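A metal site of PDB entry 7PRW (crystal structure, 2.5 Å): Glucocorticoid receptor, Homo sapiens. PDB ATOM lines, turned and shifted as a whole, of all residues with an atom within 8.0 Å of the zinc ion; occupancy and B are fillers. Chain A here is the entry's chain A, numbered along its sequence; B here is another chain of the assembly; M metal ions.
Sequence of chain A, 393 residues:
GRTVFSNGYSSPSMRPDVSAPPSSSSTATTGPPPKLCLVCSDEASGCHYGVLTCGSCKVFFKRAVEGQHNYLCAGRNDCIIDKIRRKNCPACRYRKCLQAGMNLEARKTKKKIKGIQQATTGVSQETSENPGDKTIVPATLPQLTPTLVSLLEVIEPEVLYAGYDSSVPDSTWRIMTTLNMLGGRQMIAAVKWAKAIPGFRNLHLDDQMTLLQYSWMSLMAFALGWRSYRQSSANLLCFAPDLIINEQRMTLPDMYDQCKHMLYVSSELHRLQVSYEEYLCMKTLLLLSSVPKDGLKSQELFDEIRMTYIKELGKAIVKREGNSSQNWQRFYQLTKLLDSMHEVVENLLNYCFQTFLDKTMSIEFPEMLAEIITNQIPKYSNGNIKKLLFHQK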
ATOM      1  N   LEU A  72      31.160  11.232   6.834  1.00  0.00           N
ATOM      2  CA  LEU A  72      31.397  11.004   5.405  1.00  0.00           C
ATOM      3  C   LEU A  72      30.504   9.908   4.890  1.00  0.00           C
ATOM      4  O   LEU A  72      30.083   9.014   5.644  1.00  0.00           O
ATOM      5  CB  LEU A  72      32.868  10.772   5.047  1.00  0.00           C
ATOM      6  CG  LEU A  72      33.293  11.259   3.648  1.00  0.00           C
ATOM      7  CD1 LEU A  72      33.485  12.749   3.639  1.00  0.00           C
ATOM      8  CD2 LEU A  72      34.603  10.608   3.209  1.00  0.00           C
ATOM      9  N   CYS A  73      30.145  10.007   3.615  1.00  0.00           N
ATOM     10  CA  CYS A  73      29.234   9.075   3.003  1.00  0.00           C
ATOM     11  C   CYS A  73      29.967   7.981   2.268  1.00  0.00           C
ATOM     12  O   CYS A  73      30.811   8.282   1.436  1.00  0.00           O
ATOM     13  CB  CYS A  73      28.287   9.821   2.071  1.00  0.00           C
ATOM     14  SG  CYS A  73      26.950   8.805   1.410  1.00  0.00           S
ATOM     15  N   ALA A  74      29.671   6.719   2.584  1.00  0.00           N
ATOM     16  CA  ALA A  74      30.272   5.600   1.874  1.00  0.00           C
ATOM     17  C   ALA A  74      29.630   5.427   0.481  1.00  0.00           C
ATOM     18  O   ALA A  74      30.258   4.855  -0.396  1.00  0.00           O
ATOM     19  CB  ALA A  74      30.141   4.334   2.674  1.00  0.00           C
ATOM     20  N   GLY A  75      28.389   5.890   0.287  1.00  0.00           N
ATOM     21  CA  GLY A  75      27.656   5.837  -0.973  1.00  0.00           C
ATOM     22  C   GLY A  75      27.857   7.083  -1.809  1.00  0.00           C
ATOM     23  O   GLY A  75      29.012   7.446  -2.050  1.00  0.00           O
ATOM     24  N   ARG A  76      26.773   7.752  -2.283  1.00  0.00           N
ATOM     25  CA  ARG A  76      26.936   8.955  -3.117  1.00  0.00           C
ATOM     26  C   ARG A  76      26.061  10.127  -2.712  1.00  0.00           C
ATOM     27  O   ARG A  76      25.548  10.854  -3.549  1.00  0.00           O
ATOM     28  CB  ARG A  76      26.747   8.643  -4.610  1.00  0.00           C
ATOM     29  CG  ARG A  76      27.887   7.871  -5.253  1.00  0.00           C
ATOM     30  CD  ARG A  76      27.475   7.345  -6.599  1.00  0.00           C
ATOM     31  NE  ARG A  76      28.445   6.407  -7.154  1.00  0.00           N
ATOM     32  CZ  ARG A  76      28.420   5.091  -6.943  1.00  0.00           C
ATOM     33  NH1 ARG A  76      27.505   4.558  -6.152  1.00  0.00           N
ATOM     34  NH2 ARG A  76      29.338   4.317  -7.488  1.00  0.00           N
ATOM     35  N   ASN A  77      25.929  10.336  -1.399  1.00  0.00           N
ATOM     36  CA  ASN A  77      25.140  11.399  -0.781  1.00  0.00           C
ATOM     37  C   ASN A  77      23.657  11.292  -1.092  1.00  0.00           C
ATOM     38  O   ASN A  77      22.956  12.276  -1.012  1.00  0.00           O
ATOM     39  CB  ASN A  77      25.683  12.777  -1.079  1.00  0.00           C
ATOM     40  CG  ASN A  77      26.982  13.057  -0.379  1.00  0.00           C
ATOM     41  OD1 ASN A  77      27.194  12.659   0.781  1.00  0.00           O
ATOM     42  ND2 ASN A  77      27.878  13.731  -1.054  1.00  0.00           N
ATOM     43  N   ASP A  78      23.159  10.092  -1.339  1.00  0.00           N
ATOM     44  CA  ASP A  78      21.761   9.836  -1.591  1.00  0.00           C
ATOM     45  C   ASP A  78      21.355   8.469  -1.056  1.00  0.00           C
ATOM     46  O   ASP A  78      20.667   7.711  -1.750  1.00  0.00           O
ATOM     47  CB  ASP A  78      21.472   9.958  -3.087  1.00  0.00           C
ATOM     48  CG  ASP A  78      22.382   9.155  -3.985  1.00  0.00           C
ATOM     49  OD1 ASP A  78      23.149   8.292  -3.462  1.00  0.00           O
ATOM     50  OD2 ASP A  78      22.312   9.364  -5.214  1.00  0.00           O
ATOM     51  N   CYS A  79      21.818   8.136   0.138  1.00  0.00           N
ATOM     52  CA  CYS A  79      21.482   6.863   0.752  1.00  0.00           C
ATOM     53  C   CYS A  79      20.009   6.841   1.168  1.00  0.00           C
ATOM     54  O   CYS A  79      19.392   7.904   1.349  1.00  0.00           O
ATOM     55  CB  CYS A  79      22.415   6.592   1.932  1.00  0.00           C
ATOM     56  SG  CYS A  79      24.166   6.534   1.491  1.00  0.00           S
ATOM     57  N   ILE A  80      19.415   5.633   1.249  1.00  0.00           N
ATOM     58  CA  ILE A  80      18.014   5.518   1.651  1.00  0.00           C
ATOM     59  C   ILE A  80      17.975   5.472   3.147  1.00  0.00           C
ATOM     60  O   ILE A  80      18.545   4.573   3.740  1.00  0.00           O
ATOM     61  CB  ILE A  80      17.328   4.261   1.121  1.00  0.00           C
ATOM     62  CG1 ILE A  80      17.583   4.045  -0.358  1.00  0.00           C
ATOM     63  CG2 ILE A  80      15.859   4.323   1.413  1.00  0.00           C
ATOM     64  CD1 ILE A  80      17.788   2.481  -0.683  1.00  0.00           C
ATOM     65  N   ILE A  81      17.294   6.444   3.758  1.00  0.00           N
ATOM     66  CA  ILE A  81      17.172   6.454   5.204  1.00  0.00           C
ATOM     67  C   ILE A  81      15.808   5.861   5.613  1.00  0.00           C
ATOM     68  O   ILE A  81      14.745   6.426   5.298  1.00  0.00           O
ATOM     69  CB  ILE A  81      17.472   7.826   5.847  1.00  0.00           C
ATOM     70  CG1 ILE A  81      18.769   8.427   5.277  1.00  0.00           C
ATOM     71  CG2 ILE A  81      17.533   7.695   7.364  1.00  0.00           C
ATOM     72  CD1 ILE A  81      20.019   7.612   5.510  1.00  0.00           C
ATOM     73  N   ASN A  88      23.100   3.007   9.173  1.00  0.00           N
ATOM     74  CA  ASN A  88      23.924   2.914   7.979  1.00  0.00           C
ATOM     75  C   ASN A  88      24.712   4.176   7.678  1.00  0.00           C
ATOM     76  O   ASN A  88      25.925   4.130   7.753  1.00  0.00           O
ATOM     77  CB  ASN A  88      23.076   2.536   6.775  1.00  0.00           C
ATOM     78  CG  ASN A  88      23.135   1.097   6.358  1.00  0.00           C
ATOM     79  OD1 ASN A  88      23.649   0.783   5.264  1.00  0.00           O
ATOM     80  ND2 ASN A  88      22.586   0.203   7.186  1.00  0.00           N
ATOM     81  N   CYS A  89      24.069   5.297   7.363  1.00  0.00           N
ATOM     82  CA  CYS A  89      24.795   6.496   7.009  1.00  0.00           C
ATOM     83  C   CYS A  89      24.414   7.726   7.831  1.00  0.00           C
ATOM     84  O   CYS A  89      23.338   8.306   7.671  1.00  0.00           O
ATOM     85  CB  CYS A  89      24.667   6.767   5.518  1.00  0.00           C
ATOM     86  SG  CYS A  89      25.691   8.131   4.946  1.00  0.00           S
ATOM     87  N   PRO A  90      25.334   8.169   8.698  1.00  0.00           N
ATOM     88  CA  PRO A  90      25.063   9.389   9.481  1.00  0.00           C
ATOM     89  C   PRO A  90      25.226  10.650   8.638  1.00  0.00           C
ATOM     90  O   PRO A  90      24.682  11.676   9.003  1.00  0.00           O
ATOM     91  CB  PRO A  90      26.076   9.308  10.632  1.00  0.00           C
ATOM     92  CG  PRO A  90      26.790   7.981  10.477  1.00  0.00           C
ATOM     93  CD  PRO A  90      26.655   7.605   9.027  1.00  0.00           C
ATOM     94  N   ALA A  91      25.955  10.592   7.509  1.00  0.00           N
ATOM     95  CA  ALA A  91      26.121  11.743   6.648  1.00  0.00           C
ATOM     96  C   ALA A  91      24.789  12.063   5.945  1.00  0.00           C
ATOM     97  O   ALA A  91      24.398  13.232   5.855  1.00  0.00           O
ATOM     98  CB  ALA A  91      27.219  11.483   5.629  1.00  0.00           C
ATOM     99  N   CYS A  92      24.089  11.034   5.479  1.00  0.00           N
ATOM    100  CA  CYS A  92      22.807  11.167   4.801  1.00  0.00           C
ATOM    101  C   CYS A  92      21.658  11.266   5.777  1.00  0.00           C
ATOM    102  O   CYS A  92      20.629  11.849   5.411  1.00  0.00           O
ATOM    103  CB  CYS A  92      22.589  10.051   3.787  1.00  0.00           C
ATOM    104  SG  CYS A  92      23.705  10.134   2.368  1.00  0.00           S
ATOM    105  N   ARG A  93      21.800  10.715   6.986  1.00  0.00           N
ATOM    106  CA  ARG A  93      20.749  10.879   7.979  1.00  0.00           C
ATOM    107  C   ARG A  93      20.821  12.300   8.485  1.00  0.00           C
ATOM    108  O   ARG A  93      19.780  12.935   8.535  1.00  0.00           O
ATOM    109  CB  ARG A  93      20.904   9.887   9.117  1.00  0.00           C
ATOM    110  CG  ARG A  93      19.763   9.922  10.101  1.00  0.00           C
ATOM    111  CD  ARG A  93      20.051   8.938  11.186  1.00  0.00           C
ATOM    112  NE  ARG A  93      18.955   8.703  12.114  1.00  0.00           N
ATOM    113  CZ  ARG A  93      19.015   7.863  13.151  1.00  0.00           C
ATOM    114  NH1 ARG A  93      20.128   7.190  13.390  1.00  0.00           N
ATOM    115  NH2 ARG A  93      17.975   7.722  13.961  1.00  0.00           N
ATOM    116  N   ARG A  95      21.880  14.833   6.828  1.00  0.00           N
ATOM    117  CA  ARG A  95      21.460  15.639   5.689  1.00  0.00           C
ATOM    118  C   ARG A  95      19.929  15.604   5.603  1.00  0.00           C
ATOM    119  O   ARG A  95      19.320  16.646   5.460  1.00  0.00           O
ATOM    120  CB  ARG A  95      22.109  15.125   4.392  1.00  0.00           C
ATOM    121  CG  ARG A  95      21.620  15.742   3.112  1.00  0.00           C
ATOM    122  CD  ARG A  95      22.094  17.178   2.963  1.00  0.00           C
ATOM    123  NE  ARG A  95      21.055  18.141   3.343  1.00  0.00           N
ATOM    124  CZ  ARG A  95      20.063  18.541   2.550  1.00  0.00           C
ATOM    125  NH1 ARG A  95      19.955  18.052   1.323  1.00  0.00           N
ATOM    126  NH2 ARG A  95      19.167  19.429   2.978  1.00  0.00           N
ATOM    127  N   GLN A 273      28.792  18.808  -0.479  1.00  0.00           N
ATOM    128  CA  GLN A 273      28.116  17.521  -0.308  1.00  0.00           C
ATOM    129  C   GLN A 273      27.244  17.199  -1.520  1.00  0.00           C
ATOM    130  O   GLN A 273      26.034  16.997  -1.383  1.00  0.00           O
ATOM    131  CB  GLN A 273      27.268  17.534   0.974  1.00  0.00           C
ATOM    132  CG  GLN A 273      27.912  16.884   2.152  1.00  0.00           C
ATOM    133  CD  GLN A 273      26.860  16.853   3.221  1.00  0.00           C
ATOM    134  OE1 GLN A 273      26.773  17.757   4.059  1.00  0.00           O
ATOM    135  NE2 GLN A 273      26.005  15.831   3.191  1.00  0.00           N
ATOM    136  N   ALA B  74      22.239   0.836   1.932  1.00  0.00           N
ATOM    137  CA  ALA B  74      21.477   2.068   1.730  1.00  0.00           C
ATOM    138  C   ALA B  74      21.802   2.775   0.376  1.00  0.00           C
ATOM    139  O   ALA B  74      21.058   3.654  -0.042  1.00  0.00           O
ATOM    140  CB  ALA B  74      21.678   3.019   2.891  1.00  0.00           C
ATOM    141  N   GLY B  75      22.860   2.348  -0.305  1.00  0.00           N
ATOM    142  CA  GLY B  75      23.295   2.927  -1.573  1.00  0.00           C
ATOM    143  C   GLY B  75      23.066   2.025  -2.763  1.00  0.00           C
ATOM    144  O   GLY B  75      21.928   1.619  -3.010  1.00  0.00           O
ATOM    145  N   CYS B  79      29.333   0.598  -1.782  1.00  0.00           N
ATOM    146  CA  CYS B  79      29.807   1.558  -0.798  1.00  0.00           C
ATOM    147  C   CYS B  79      31.298   1.408  -0.564  1.00  0.00           C
ATOM    148  O   CYS B  79      31.827   0.297  -0.636  1.00  0.00           O
ATOM    149  CB  CYS B  79      29.043   1.438   0.514  1.00  0.00           C
ATOM    150  SG  CYS B  79      27.256   1.563   0.339  1.00  0.00           S
ATOM    151  N   ASN B  88      29.953   2.103   8.410  1.00  0.00           N
ATOM    152  CA  ASN B  88      28.795   2.556   7.662  1.00  0.00           C
ATOM    153  C   ASN B  88      27.996   1.462   7.003  1.00  0.00           C
ATOM    154  O   ASN B  88      26.873   1.246   7.457  1.00  0.00           O
ATOM    155  CB  ASN B  88      29.161   3.653   6.663  1.00  0.00           C
ATOM    156  CG  ASN B  88      29.529   4.943   7.328  1.00  0.00           C
ATOM    157  OD1 ASN B  88      29.418   5.110   8.564  1.00  0.00           O
ATOM    158  ND2 ASN B  88      29.972   5.894   6.522  1.00  0.00           N
HETATM  159 ZN    ZN M   1      25.122   8.208   2.602  1.00  0.00          ZN
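SG of Cys 73 lies close to N of Asn 77, 3.4 Å away. The side-chain sulfur (SG) of Cys 73 sits close to the backbone NH (N) of Gly 75 of chain A (3.4 Å). N of Asp 78 sits close to SG of Cys 92. The side-chain sulfur (SG) of Cys 89 sits close to the backbone NH (N) of Ala 91.
Along chain A the residues within 4 Å of the zinc ion span positions 73 to 92. The nearest printed residue that does not touch the zinc ion is Asn 77 (4.6 Å).
SG of Cys 79 of chain A is bound to the zinc ion, at 2.2 Å. The zinc ion is bound by the side-chain sulfur (SG) of Cys 73, at 2.3 Å. SG of Cys 92 binds the zinc ion, at 2.4 Å. SG of Cys 89 binds the zinc ion. The zinc ion has four donor atoms within binding distance.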
